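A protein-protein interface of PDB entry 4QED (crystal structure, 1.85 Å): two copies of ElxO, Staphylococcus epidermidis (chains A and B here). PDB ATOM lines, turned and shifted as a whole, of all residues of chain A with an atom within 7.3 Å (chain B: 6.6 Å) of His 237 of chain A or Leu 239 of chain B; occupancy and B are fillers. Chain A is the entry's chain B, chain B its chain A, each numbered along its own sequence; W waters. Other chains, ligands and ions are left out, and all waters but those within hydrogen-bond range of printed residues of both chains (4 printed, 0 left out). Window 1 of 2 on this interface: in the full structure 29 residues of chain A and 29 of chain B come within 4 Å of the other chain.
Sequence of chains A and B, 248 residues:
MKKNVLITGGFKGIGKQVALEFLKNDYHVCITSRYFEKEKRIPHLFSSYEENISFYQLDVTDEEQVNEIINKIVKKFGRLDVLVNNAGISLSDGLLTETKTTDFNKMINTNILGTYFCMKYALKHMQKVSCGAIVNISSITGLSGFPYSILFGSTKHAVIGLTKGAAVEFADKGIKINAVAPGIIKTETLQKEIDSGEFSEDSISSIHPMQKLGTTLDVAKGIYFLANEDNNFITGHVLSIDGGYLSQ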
ATOM      1  N   VAL A 135      31.190 -23.902 -29.669  1.00  0.00           N
ATOM      2  CA  VAL A 135      30.328 -23.230 -28.703  1.00  0.00           C
ATOM      3  C   VAL A 135      30.957 -21.880 -28.366  1.00  0.00           C
ATOM      4  O   VAL A 135      32.087 -21.805 -27.890  1.00  0.00           O
ATOM      5  CB  VAL A 135      30.052 -24.076 -27.432  1.00  0.00           C
ATOM      6  CG1 VAL A 135      28.967 -23.416 -26.583  1.00  0.00           C
ATOM      7  CG2 VAL A 135      29.614 -25.495 -27.788  1.00  0.00           C
ATOM      8  N   ASN A 136      30.220 -20.815 -28.650  1.00  0.00           N
ATOM      9  CA  ASN A 136      30.658 -19.472 -28.307  1.00  0.00           C
ATOM     10  C   ASN A 136      30.045 -19.060 -26.989  1.00  0.00           C
ATOM     11  O   ASN A 136      28.988 -19.557 -26.617  1.00  0.00           O
ATOM     12  CB  ASN A 136      30.272 -18.494 -29.413  1.00  0.00           C
ATOM     13  CG  ASN A 136      31.030 -18.762 -30.698  1.00  0.00           C
ATOM     14  OD1 ASN A 136      32.142 -19.274 -30.662  1.00  0.00           O
ATOM     15  ND2 ASN A 136      30.437 -18.418 -31.838  1.00  0.00           N
ATOM     16  N   ILE A 160      26.659 -13.451 -30.903  1.00  0.00           N
ATOM     17  CA  ILE A 160      25.462 -14.151 -31.369  1.00  0.00           C
ATOM     18  C   ILE A 160      25.342 -14.075 -32.907  1.00  0.00           C
ATOM     19  O   ILE A 160      25.030 -15.080 -33.565  1.00  0.00           O
ATOM     20  CB  ILE A 160      24.206 -13.651 -30.631  1.00  0.00           C
ATOM     21  CG1 ILE A 160      24.299 -14.061 -29.147  1.00  0.00           C
ATOM     22  CG2 ILE A 160      22.931 -14.187 -31.271  1.00  0.00           C
ATOM     23  CD1 ILE A 160      23.150 -13.602 -28.274  1.00  0.00           C
ATOM     24  N   THR A 163      27.635 -16.516 -34.381  1.00  0.00           N
ATOM     25  CA  THR A 163      27.116 -17.838 -34.062  1.00  0.00           C
ATOM     26  C   THR A 163      26.014 -18.266 -35.025  1.00  0.00           C
ATOM     27  O   THR A 163      26.103 -19.331 -35.631  1.00  0.00           O
ATOM     28  CB  THR A 163      26.586 -17.904 -32.615  1.00  0.00           C
ATOM     29  OG1 THR A 163      27.626 -17.498 -31.720  1.00  0.00           O
ATOM     30  CG2 THR A 163      26.151 -19.328 -32.271  1.00  0.00           C
ATOM     31  N   LYS A 164      24.978 -17.438 -35.148  1.00  0.00           N
ATOM     32  CA  LYS A 164      23.846 -17.746 -36.008  1.00  0.00           C
ATOM     33  C   LYS A 164      24.245 -17.745 -37.483  1.00  0.00           C
ATOM     34  O   LYS A 164      23.823 -18.625 -38.231  1.00  0.00           O
ATOM     35  CB  LYS A 164      22.697 -16.759 -35.786  1.00  0.00           C
ATOM     36  CG  LYS A 164      22.047 -16.824 -34.415  1.00  0.00           C
ATOM     37  CD  LYS A 164      20.841 -15.905 -34.419  1.00  0.00           C
ATOM     38  CE  LYS A 164      19.995 -16.054 -33.170  1.00  0.00           C
ATOM     39  NZ  LYS A 164      18.753 -15.248 -33.348  1.00  0.00           N
ATOM     40  N   ALA A 167      26.346 -20.844 -38.186  1.00  0.00           N
ATOM     41  CA  ALA A 167      25.467 -22.007 -38.069  1.00  0.00           C
ATOM     42  C   ALA A 167      24.712 -22.287 -39.363  1.00  0.00           C
ATOM     43  O   ALA A 167      24.718 -23.427 -39.860  1.00  0.00           O
ATOM     44  CB  ALA A 167      24.490 -21.844 -36.916  1.00  0.00           C
ATOM     45  N   ILE A 177      27.017 -25.197 -34.428  1.00  0.00           N
ATOM     46  CA  ILE A 177      27.590 -23.962 -33.935  1.00  0.00           C
ATOM     47  C   ILE A 177      26.527 -23.280 -33.098  1.00  0.00           C
ATOM     48  O   ILE A 177      25.478 -22.866 -33.604  1.00  0.00           O
ATOM     49  CB  ILE A 177      28.060 -23.042 -35.092  1.00  0.00           C
ATOM     50  CG1 ILE A 177      29.017 -23.801 -36.023  1.00  0.00           C
ATOM     51  CG2 ILE A 177      28.713 -21.782 -34.532  1.00  0.00           C
ATOM     52  CD1 ILE A 177      29.414 -23.056 -37.277  1.00  0.00           C
ATOM     53  N   ASN A 178      26.804 -23.174 -31.807  1.00  0.00           N
ATOM     54  CA  ASN A 178      25.824 -22.659 -30.868  1.00  0.00           C
ATOM     55  C   ASN A 178      26.513 -21.721 -29.903  1.00  0.00           C
ATOM     56  O   ASN A 178      27.731 -21.581 -29.933  1.00  0.00           O
ATOM     57  CB  ASN A 178      25.165 -23.798 -30.087  1.00  0.00           C
ATOM     58  CG  ASN A 178      24.320 -24.697 -30.967  1.00  0.00           C
ATOM     59  OD1 ASN A 178      23.199 -24.358 -31.329  1.00  0.00           O
ATOM     60  ND2 ASN A 178      24.857 -25.850 -31.303  1.00  0.00           N
ATOM     61  N   ALA A 179      25.725 -21.076 -29.053  1.00  0.00           N
ATOM     62  CA  ALA A 179      26.286 -20.195 -28.041  1.00  0.00           C
ATOM     63  C   ALA A 179      25.591 -20.405 -26.707  1.00  0.00           C
ATOM     64  O   ALA A 179      24.470 -20.931 -26.638  1.00  0.00           O
ATOM     65  CB  ALA A 179      26.189 -18.739 -28.485  1.00  0.00           C
ATOM     66  N   VAL A 180      26.266 -20.013 -25.635  1.00  0.00           N
ATOM     67  CA  VAL A 180      25.612 -19.952 -24.337  1.00  0.00           C
ATOM     68  C   VAL A 180      25.539 -18.490 -23.921  1.00  0.00           C
ATOM     69  O   VAL A 180      26.420 -17.706 -24.268  1.00  0.00           O
ATOM     70  CB  VAL A 180      26.339 -20.777 -23.258  1.00  0.00           C
ATOM     71  CG1 VAL A 180      26.204 -22.273 -23.536  1.00  0.00           C
ATOM     72  CG2 VAL A 180      27.805 -20.368 -23.142  1.00  0.00           C
ATOM     73  N   PHE A 225      26.814 -29.906 -23.167  1.00  0.00           N
ATOM     74  CA  PHE A 225      25.601 -30.402 -23.827  1.00  0.00           C
ATOM     75  C   PHE A 225      25.571 -30.026 -25.316  1.00  0.00           C
ATOM     76  O   PHE A 225      25.223 -30.846 -26.163  1.00  0.00           O
ATOM     77  CB  PHE A 225      24.337 -29.875 -23.134  1.00  0.00           C
ATOM     78  CG  PHE A 225      23.075 -30.137 -23.909  1.00  0.00           C
ATOM     79  CD1 PHE A 225      22.548 -31.428 -23.980  1.00  0.00           C
ATOM     80  CD2 PHE A 225      22.437 -29.112 -24.600  1.00  0.00           C
ATOM     81  CE1 PHE A 225      21.405 -31.685 -24.717  1.00  0.00           C
ATOM     82  CE2 PHE A 225      21.284 -29.365 -25.340  1.00  0.00           C
ATOM     83  CZ  PHE A 225      20.770 -30.655 -25.393  1.00  0.00           C
ATOM     84  N   LEU A 226      25.932 -28.782 -25.621  1.00  0.00           N
ATOM     85  CA  LEU A 226      25.878 -28.299 -27.007  1.00  0.00           C
ATOM     86  C   LEU A 226      27.016 -28.837 -27.854  1.00  0.00           C
ATOM     87  O   LEU A 226      26.913 -28.848 -29.080  1.00  0.00           O
ATOM     88  CB  LEU A 226      25.853 -26.767 -27.063  1.00  0.00           C
ATOM     89  CG  LEU A 226      24.652 -26.052 -26.426  1.00  0.00           C
ATOM     90  CD1 LEU A 226      24.947 -24.581 -26.185  1.00  0.00           C
ATOM     91  CD2 LEU A 226      23.398 -26.199 -27.269  1.00  0.00           C
ATOM     92  N   ILE A 234      20.922 -29.634 -32.906  1.00  0.00           N
ATOM     93  CA  ILE A 234      20.875 -28.294 -32.323  1.00  0.00           C
ATOM     94  C   ILE A 234      22.006 -27.465 -32.923  1.00  0.00           C
ATOM     95  O   ILE A 234      23.191 -27.754 -32.718  1.00  0.00           O
ATOM     96  CB  ILE A 234      20.909 -28.312 -30.773  1.00  0.00           C
ATOM     97  CG1 ILE A 234      19.728 -29.143 -30.236  1.00  0.00           C
ATOM     98  CG2 ILE A 234      20.886 -26.882 -30.225  1.00  0.00           C
ATOM     99  CD1 ILE A 234      19.827 -29.545 -28.770  1.00  0.00           C
ATOM    100  N   THR A 235      21.625 -26.453 -33.697  1.00  0.00           N
ATOM    101  CA  THR A 235      22.593 -25.505 -34.253  1.00  0.00           C
ATOM    102  C   THR A 235      21.963 -24.115 -34.405  1.00  0.00           C
ATOM    103  O   THR A 235      20.738 -23.991 -34.533  1.00  0.00           O
ATOM    104  CB  THR A 235      23.223 -26.029 -35.570  1.00  0.00           C
ATOM    105  OG1 THR A 235      24.404 -25.282 -35.869  1.00  0.00           O
ATOM    106  CG2 THR A 235      22.237 -25.937 -36.731  1.00  0.00           C
ATOM    107  N   GLY A 236      22.799 -23.076 -34.350  1.00  0.00           N
ATOM    108  CA  GLY A 236      22.320 -21.691 -34.371  1.00  0.00           C
ATOM    109  C   GLY A 236      21.564 -21.228 -33.133  1.00  0.00           C
ATOM    110  O   GLY A 236      20.911 -20.175 -33.151  1.00  0.00           O
ATOM    111  N   HIS A 237      21.668 -21.987 -32.048  1.00  0.00           N
ATOM    112  CA  HIS A 237      20.885 -21.704 -30.845  1.00  0.00           C
ATOM    113  C   HIS A 237      21.715 -21.010 -29.780  1.00  0.00           C
ATOM    114  O   HIS A 237      22.919 -21.247 -29.666  1.00  0.00           O
ATOM    115  CB  HIS A 237      20.294 -22.987 -30.268  1.00  0.00           C
ATOM    116  CG  HIS A 237      19.400 -22.760 -29.087  1.00  0.00           C
ATOM    117  ND1 HIS A 237      18.202 -22.084 -29.179  1.00  0.00           N
ATOM    118  CD2 HIS A 237      19.540 -23.101 -27.784  1.00  0.00           C
ATOM    119  CE1 HIS A 237      17.637 -22.030 -27.987  1.00  0.00           C
ATOM    120  NE2 HIS A 237      18.425 -22.645 -27.124  1.00  0.00           N
ATOM    121  N   VAL A 238      21.053 -20.162 -28.997  1.00  0.00           N
ATOM    122  CA  VAL A 238      21.685 -19.506 -27.872  1.00  0.00           C
ATOM    123  C   VAL A 238      21.001 -20.010 -26.600  1.00  0.00           C
ATOM    124  O   VAL A 238      19.843 -19.701 -26.343  1.00  0.00           O
ATOM    125  CB  VAL A 238      21.569 -17.969 -27.961  1.00  0.00           C
ATOM    126  CG1 VAL A 238      22.346 -17.320 -26.823  1.00  0.00           C
ATOM    127  CG2 VAL A 238      22.058 -17.458 -29.310  1.00  0.00           C
ATOM    128  N   LEU A 239      21.727 -20.806 -25.828  1.00  0.00           N
ATOM    129  CA  LEU A 239      21.196 -21.402 -24.610  1.00  0.00           C
ATOM    130  C   LEU A 239      21.398 -20.440 -23.439  1.00  0.00           C
ATOM    131  O   LEU A 239      22.533 -20.161 -23.072  1.00  0.00           O
ATOM    132  CB  LEU A 239      21.904 -22.739 -24.333  1.00  0.00           C
ATOM    133  CG  LEU A 239      21.520 -23.512 -23.058  1.00  0.00           C
ATOM    134  CD1 LEU A 239      20.055 -23.939 -23.080  1.00  0.00           C
ATOM    135  CD2 LEU A 239      22.436 -24.719 -22.882  1.00  0.00           C
ATOM    136  N   SER A 240      20.308 -19.951 -22.853  1.00  0.00           N
ATOM    137  CA  SER A 240      20.397 -19.022 -21.722  1.00  0.00           C
ATOM    138  C   SER A 240      20.679 -19.807 -20.454  1.00  0.00           C
ATOM    139  O   SER A 240      20.011 -20.791 -20.178  1.00  0.00           O
ATOM    140  CB  SER A 240      19.097 -18.241 -21.554  1.00  0.00           C
ATOM    141  OG  SER A 240      18.744 -17.594 -22.762  1.00  0.00           O
ATOM    142  N   LEU B 143       7.330 -20.238 -32.233  1.00  0.00           N
ATOM    143  CA  LEU B 143       8.278 -19.111 -32.277  1.00  0.00           C
ATOM    144  C   LEU B 143       8.366 -18.460 -33.661  1.00  0.00           C
ATOM    145  O   LEU B 143       9.188 -17.560 -33.887  1.00  0.00           O
ATOM    146  CB  LEU B 143       9.674 -19.585 -31.860  1.00  0.00           C
ATOM    147  CG  LEU B 143       9.897 -19.787 -30.358  1.00  0.00           C
ATOM    148  CD1 LEU B 143      11.062 -20.723 -30.074  1.00  0.00           C
ATOM    149  CD2 LEU B 143      10.106 -18.453 -29.660  1.00  0.00           C
ATOM    150  N   ASN B 178      10.938 -25.272 -18.317  1.00  0.00           N
ATOM    151  CA  ASN B 178      11.507 -24.977 -19.632  1.00  0.00           C
ATOM    152  C   ASN B 178      10.691 -25.662 -20.716  1.00  0.00           C
ATOM    153  O   ASN B 178       9.794 -26.454 -20.431  1.00  0.00           O
ATOM    154  CB  ASN B 178      12.962 -25.457 -19.722  1.00  0.00           C
ATOM    155  CG  ASN B 178      13.873 -24.750 -18.737  1.00  0.00           C
ATOM    156  OD1 ASN B 178      14.224 -25.301 -17.686  1.00  0.00           O
ATOM    157  ND2 ASN B 178      14.254 -23.541 -19.064  1.00  0.00           N
ATOM    158  N   ALA B 179      10.998 -25.342 -21.968  1.00  0.00           N
ATOM    159  CA  ALA B 179      10.308 -25.976 -23.082  1.00  0.00           C
ATOM    160  C   ALA B 179      11.319 -26.383 -24.131  1.00  0.00           C
ATOM    161  O   ALA B 179      12.427 -25.840 -24.182  1.00  0.00           O
ATOM    162  CB  ALA B 179       9.270 -25.025 -23.678  1.00  0.00           C
ATOM    163  N   VAL B 180      10.951 -27.357 -24.958  1.00  0.00           N
ATOM    164  CA  VAL B 180      11.716 -27.617 -26.171  1.00  0.00           C
ATOM    165  C   VAL B 180      10.860 -27.213 -27.369  1.00  0.00           C
ATOM    166  O   VAL B 180       9.631 -27.301 -27.302  1.00  0.00           O
ATOM    167  CB  VAL B 180      12.164 -29.086 -26.283  1.00  0.00           C
ATOM    168  CG1 VAL B 180      13.220 -29.389 -25.227  1.00  0.00           C
ATOM    169  CG2 VAL B 180      10.965 -30.037 -26.165  1.00  0.00           C
ATOM    170  N   ALA B 181      11.509 -26.748 -28.436  1.00  0.00           N
ATOM    171  CA  ALA B 181      10.816 -26.375 -29.670  1.00  0.00           C
ATOM    172  C   ALA B 181      11.358 -27.220 -30.810  1.00  0.00           C
ATOM    173  O   ALA B 181      12.332 -26.837 -31.452  1.00  0.00           O
ATOM    174  CB  ALA B 181      11.002 -24.892 -29.970  1.00  0.00           C
ATOM    175  N   PRO B 182      10.757 -28.404 -31.036  1.00  0.00           N
ATOM    176  CA  PRO B 182      11.250 -29.269 -32.106  1.00  0.00           C
ATOM    177  C   PRO B 182      10.888 -28.745 -33.495  1.00  0.00           C
ATOM    178  O   PRO B 182       9.846 -28.103 -33.667  1.00  0.00           O
ATOM    179  CB  PRO B 182      10.541 -30.607 -31.843  1.00  0.00           C
ATOM    180  CG  PRO B 182      10.031 -30.529 -30.431  1.00  0.00           C
ATOM    181  CD  PRO B 182       9.712 -29.066 -30.234  1.00  0.00           C
ATOM    182  N   LYS B 221      16.815 -36.171 -25.779  1.00  0.00           N
ATOM    183  CA  LYS B 221      18.071 -35.705 -25.186  1.00  0.00           C
ATOM    184  C   LYS B 221      17.961 -34.272 -24.669  1.00  0.00           C
ATOM    185  O   LYS B 221      18.474 -33.965 -23.593  1.00  0.00           O
ATOM    186  CB  LYS B 221      19.219 -35.798 -26.198  1.00  0.00           C
ATOM    187  CG  LYS B 221      19.591 -37.228 -26.578  1.00  0.00           C
ATOM    188  CD  LYS B 221      20.637 -37.776 -25.642  1.00  0.00           C
ATOM    189  CE  LYS B 221      21.043 -39.197 -25.998  1.00  0.00           C
ATOM    190  NZ  LYS B 221      21.835 -39.695 -24.847  1.00  0.00           N
ATOM    191  N   GLY B 222      17.299 -33.408 -25.439  1.00  0.00           N
ATOM    192  CA  GLY B 222      17.107 -32.012 -25.039  1.00  0.00           C
ATOM    193  C   GLY B 222      16.251 -31.927 -23.787  1.00  0.00           C
ATOM    194  O   GLY B 222      16.579 -31.215 -22.827  1.00  0.00           O
ATOM    195  N   ILE B 223      15.137 -32.656 -23.804  1.00  0.00           N
ATOM    196  CA  ILE B 223      14.248 -32.729 -22.656  1.00  0.00           C
ATOM    197  C   ILE B 223      14.990 -33.223 -21.415  1.00  0.00           C
ATOM    198  O   ILE B 223      14.865 -32.637 -20.330  1.00  0.00           O
ATOM    199  CB  ILE B 223      13.021 -33.623 -22.967  1.00  0.00           C
ATOM    200  CG1 ILE B 223      12.119 -32.930 -24.000  1.00  0.00           C
ATOM    201  CG2 ILE B 223      12.230 -33.962 -21.701  1.00  0.00           C
ATOM    202  CD1 ILE B 223      10.956 -33.784 -24.486  1.00  0.00           C
ATOM    203  N   PHE B 225      18.231 -33.125 -20.746  1.00  0.00           N
ATOM    204  CA  PHE B 225      19.169 -32.099 -20.295  1.00  0.00           C
ATOM    205  C   PHE B 225      18.484 -31.037 -19.425  1.00  0.00           C
ATOM    206  O   PHE B 225      19.027 -30.637 -18.410  1.00  0.00           O
ATOM    207  CB  PHE B 225      19.899 -31.449 -21.477  1.00  0.00           C
ATOM    208  CG  PHE B 225      20.634 -30.188 -21.115  1.00  0.00           C
ATOM    209  CD1 PHE B 225      21.858 -30.243 -20.444  1.00  0.00           C
ATOM    210  CD2 PHE B 225      20.103 -28.944 -21.442  1.00  0.00           C
ATOM    211  CE1 PHE B 225      22.526 -29.082 -20.094  1.00  0.00           C
ATOM    212  CE2 PHE B 225      20.775 -27.777 -21.096  1.00  0.00           C
ATOM    213  CZ  PHE B 225      21.987 -27.847 -20.429  1.00  0.00           C
ATOM    214  N   LEU B 226      17.298 -30.587 -19.835  1.00  0.00           N
ATOM    215  CA  LEU B 226      16.567 -29.542 -19.107  1.00  0.00           C
ATOM    216  C   LEU B 226      15.961 -30.044 -17.792  1.00  0.00           C
ATOM    217  O   LEU B 226      15.699 -29.253 -16.886  1.00  0.00           O
ATOM    218  CB  LEU B 226      15.479 -28.920 -19.993  1.00  0.00           C
ATOM    219  CG  LEU B 226      15.966 -28.157 -21.234  1.00  0.00           C
ATOM    220  CD1 LEU B 226      14.807 -27.891 -22.185  1.00  0.00           C
ATOM    221  CD2 LEU B 226      16.669 -26.862 -20.842  1.00  0.00           C
ATOM    222  N   HIS B 237      13.389 -21.077 -20.385  1.00  0.00           N
ATOM    223  CA  HIS B 237      14.074 -21.127 -21.681  1.00  0.00           C
ATOM    224  C   HIS B 237      13.357 -22.069 -22.632  1.00  0.00           C
ATOM    225  O   HIS B 237      12.799 -23.079 -22.206  1.00  0.00           O
ATOM    226  CB  HIS B 237      15.526 -21.585 -21.504  1.00  0.00           C
ATOM    227  CG  HIS B 237      16.317 -21.556 -22.774  1.00  0.00           C
ATOM    228  ND1 HIS B 237      16.639 -20.381 -23.415  1.00  0.00           N
ATOM    229  CD2 HIS B 237      16.808 -22.555 -23.543  1.00  0.00           C
ATOM    230  CE1 HIS B 237      17.316 -20.657 -24.518  1.00  0.00           C
ATOM    231  NE2 HIS B 237      17.428 -21.968 -24.619  1.00  0.00           N
ATOM    232  N   VAL B 238      13.420 -21.745 -23.921  1.00  0.00           N
ATOM    233  CA  VAL B 238      12.897 -22.610 -24.968  1.00  0.00           C
ATOM    234  C   VAL B 238      14.080 -23.065 -25.809  1.00  0.00           C
ATOM    235  O   VAL B 238      14.688 -22.265 -26.510  1.00  0.00           O
ATOM    236  CB  VAL B 238      11.906 -21.848 -25.875  1.00  0.00           C
ATOM    237  CG1 VAL B 238      11.259 -22.805 -26.876  1.00  0.00           C
ATOM    238  CG2 VAL B 238      10.858 -21.137 -25.039  1.00  0.00           C
ATOM    239  N   LEU B 239      14.393 -24.352 -25.716  1.00  0.00           N
ATOM    240  CA  LEU B 239      15.501 -24.959 -26.414  1.00  0.00           C
ATOM    241  C   LEU B 239      15.070 -25.411 -27.807  1.00  0.00           C
ATOM    242  O   LEU B 239      14.247 -26.313 -27.940  1.00  0.00           O
ATOM    243  CB  LEU B 239      16.023 -26.151 -25.593  1.00  0.00           C
ATOM    244  CG  LEU B 239      17.153 -26.998 -26.186  1.00  0.00           C
ATOM    245  CD1 LEU B 239      18.435 -26.191 -26.328  1.00  0.00           C
ATOM    246  CD2 LEU B 239      17.397 -28.223 -25.320  1.00  0.00           C
ATOM    247  N   SER B 240      15.621 -24.778 -28.838  1.00  0.00           N
ATOM    248  CA  SER B 240      15.304 -25.147 -30.221  1.00  0.00           C
ATOM    249  C   SER B 240      16.013 -26.438 -30.594  1.00  0.00           C
ATOM    250  O   SER B 240      17.212 -26.562 -30.387  1.00  0.00           O
ATOM    251  CB  SER B 240      15.727 -24.033 -31.168  1.00  0.00           C
ATOM    252  OG  SER B 240      15.209 -22.796 -30.732  1.00  0.00           O
ATOM    253  N   ILE B 241      15.268 -27.404 -31.125  1.00  0.00           N
ATOM    254  CA  ILE B 241      15.848 -28.678 -31.555  1.00  0.00           C
ATOM    255  C   ILE B 241      15.360 -28.846 -32.997  1.00  0.00           C
ATOM    256  O   ILE B 241      14.403 -29.561 -33.270  1.00  0.00           O
ATOM    257  CB  ILE B 241      15.436 -29.848 -30.617  1.00  0.00           C
ATOM    258  CG1 ILE B 241      15.685 -29.475 -29.136  1.00  0.00           C
ATOM    259  CG2 ILE B 241      16.207 -31.117 -30.958  1.00  0.00           C
ATOM    260  CD1 ILE B 241      15.360 -30.570 -28.127  1.00  0.00           C
ATOM    261  N   ASP B 242      16.019 -28.138 -33.908  1.00  0.00           N
ATOM    262  CA  ASP B 242      15.400 -27.788 -35.186  1.00  0.00           C
ATOM    263  C   ASP B 242      16.356 -27.708 -36.370  1.00  0.00           C
ATOM    264  O   ASP B 242      16.009 -27.133 -37.415  1.00  0.00           O
ATOM    265  CB  ASP B 242      14.634 -26.462 -35.034  1.00  0.00           C
ATOM    266  CG  ASP B 242      15.554 -25.252 -34.851  1.00  0.00           C
ATOM    267  OD1 ASP B 242      16.788 -25.405 -34.739  1.00  0.00           O
ATOM    268  OD2 ASP B 242      15.027 -24.123 -34.834  1.00  0.00           O
ATOM    269  N   GLY B 244      18.708 -25.852 -36.975  1.00  0.00           N
ATOM    270  CA  GLY B 244      19.012 -24.464 -37.347  1.00  0.00           C
ATOM    271  C   GLY B 244      17.835 -23.640 -37.842  1.00  0.00           C
ATOM    272  O   GLY B 244      18.007 -22.475 -38.185  1.00  0.00           O
ATOM    273  N   SER B 247      17.244 -20.100 -36.422  1.00  0.00           N
ATOM    274  CA  SER B 247      18.404 -19.208 -36.511  1.00  0.00           C
ATOM    275  C   SER B 247      18.485 -18.451 -37.839  1.00  0.00           C
ATOM    276  O   SER B 247      19.287 -17.527 -37.973  1.00  0.00           O
ATOM    277  CB  SER B 247      19.698 -19.977 -36.281  1.00  0.00           C
ATOM    278  OG  SER B 247      19.970 -20.849 -37.368  1.00  0.00           O
HETATM  279  O   HOH W   1      18.104 -22.851 -34.428  1.00  0.00           O
HETATM  280  O   HOH W   2      17.358 -21.338 -32.096  1.00  0.00           O
HETATM  281  O   HOH W   3      15.864 -17.883 -21.981  1.00  0.00           O
HETATM  282  O   HOH W   4      18.590 -25.941 -32.779  1.00  0.00           O
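Of the 19 printed residues of chain A, 8 touch a printed residue of chain B.
Printed residues of chain A that touch a printed residue of chain B: Phe 225, Ile 234, Thr 235, Gly 236, His 237, Val 238, Leu 239 and Ser 240.
Hydrophobic or aromatic side chains of chain A that line the printed part of chain B: Phe 225, Ile 234, His 237 and Leu 239.
Printed residues of chain B that touch a printed residue of chain A: Lys 221, Gly 222, Phe 225, His 237, Val 238, Leu 239, Ser 240, Gly 244 and Ser 247.
CE1 of Phe 225 of chain A touches O of Lys 221 of chain B, 3.9 Å away.
Phe 225 of chain A touches Gly 222 of chain B (CZ to CA, 3.9 Å).
CE1 of Phe 225 of chain A touches CB of Phe 225 of chain B, 3.6 Å away.
Ile 234 of chain A touches Ser 240 of chain B (CG1 to O, 3.6 Å).
Gly 244 of chain B touches Thr 235 of chain A.
CE1 of His 237 of chain A touches O of Val 238 of chain B (3.3 Å).
His 237 of chain A touches Leu 239 of chain B.
His 237 of chain B touches Val 238 of chain A.
Leu 239 of chain A touches Phe 225 of chain B.
CD2 of His 237 of chain B touches CD1 of Leu 239 of chain A, at 3.6 Å.
Water W4 lies within hydrogen-bond range of OD1 of Asp 242 of chain B (2.7 Å), O of Ser 240 of chain B (2.8 Å) and N of Thr 235 of chain A (3.2 Å).
Water W1 lies within hydrogen-bond range of O of Thr 235 of chain A (2.9 Å) and OD1 of Asp 242 of chain B (2.9 Å).
Water W2 lies within hydrogen-bond range of OG of Ser 240 of chain B (2.9 Å) and ND1 of His 237 of chain A (3.1 Å).
Water W3 bridges a ring nitrogen (ND1) of His 237 of chain B (3.0 Å) and the side-chain hydroxyl of Ser 240 of chain A (3.0 Å).
His 237 of chain B touches its own counterpart, His 237 of chain A.
His 237 of chain A touches Leu 239 of chain B, and with the chains exchanged Leu 239 of chain A touches His 237 of chain B.
His 237 of chain A touches Ser 240 of chain B, and with the chains exchanged Ser 240 of chain A touches His 237 of chain B.
Leu 239 of chain A touches Phe 225 of chain B, but with the chains exchanged Phe 225 of chain A does not touch Leu 239 of chain B (4.1 Å).
9 positions are printed for both chains.
His 237 of chain A touches four residues of chain B.
Of chain A, only His 237 comes within 4 Å of Leu 239 of chain B.
Printed residues of chain A within 4 Å of His 237 of chain B: His 237 (2.8 Å), Val 238 (3.3 Å), Leu 239 (3.6 Å) and Ser 240 (3.5 Å).
Of the printed residues of chain B, Val 238 of chain A touches His 237.
Printed residues of chain B within 4 Å of Thr 235 of chain A: Gly 244 (3.3 Å).
Ala 181 of chain B touches none of the printed residues of chain A.
Ile 241 of chain B touches none of the printed residues of chain A.
The nearest printed residue of chain A that does not touch Gly 222 of chain B is Ile 234 of chain A (5.2 Å).
The backbone NH of Ala 179 of chain B lies within hydrogen-bond range of the backbone carbonyl oxygen of His 237 of chain B, at 2.9 Å.
O of Ala 179 of chain B sits at hydrogen-bond distance from N of Leu 239 of chain B (2.9 Å).
O of Gly 244 of chain B lies within hydrogen-bond range of OG of Ser 247 of chain B, 2.7 Å away.
O of Ile 177 of chain A lies within hydrogen-bond range of N of Gly 236 of chain A (2.8 Å).
The backbone carbonyl oxygen (O) of Ile 234 of chain A is in hydrogen-bond range of the side-chain amide nitrogen (ND2) of Asn 178 of chain A (2.9 Å).
N of Ala 179 of chain A is in hydrogen-bond range of O of His 237 of chain A (2.9 Å).
A ring nitrogen (NE2) of His 237 of chain A lies within hydrogen-bond range of a ring nitrogen (NE2) of His 237 of chain B (2.8 Å).
ND1 of His 237 of chain A lies within hydrogen-bond range of OG of Ser 240 of chain B (3.4 Å).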
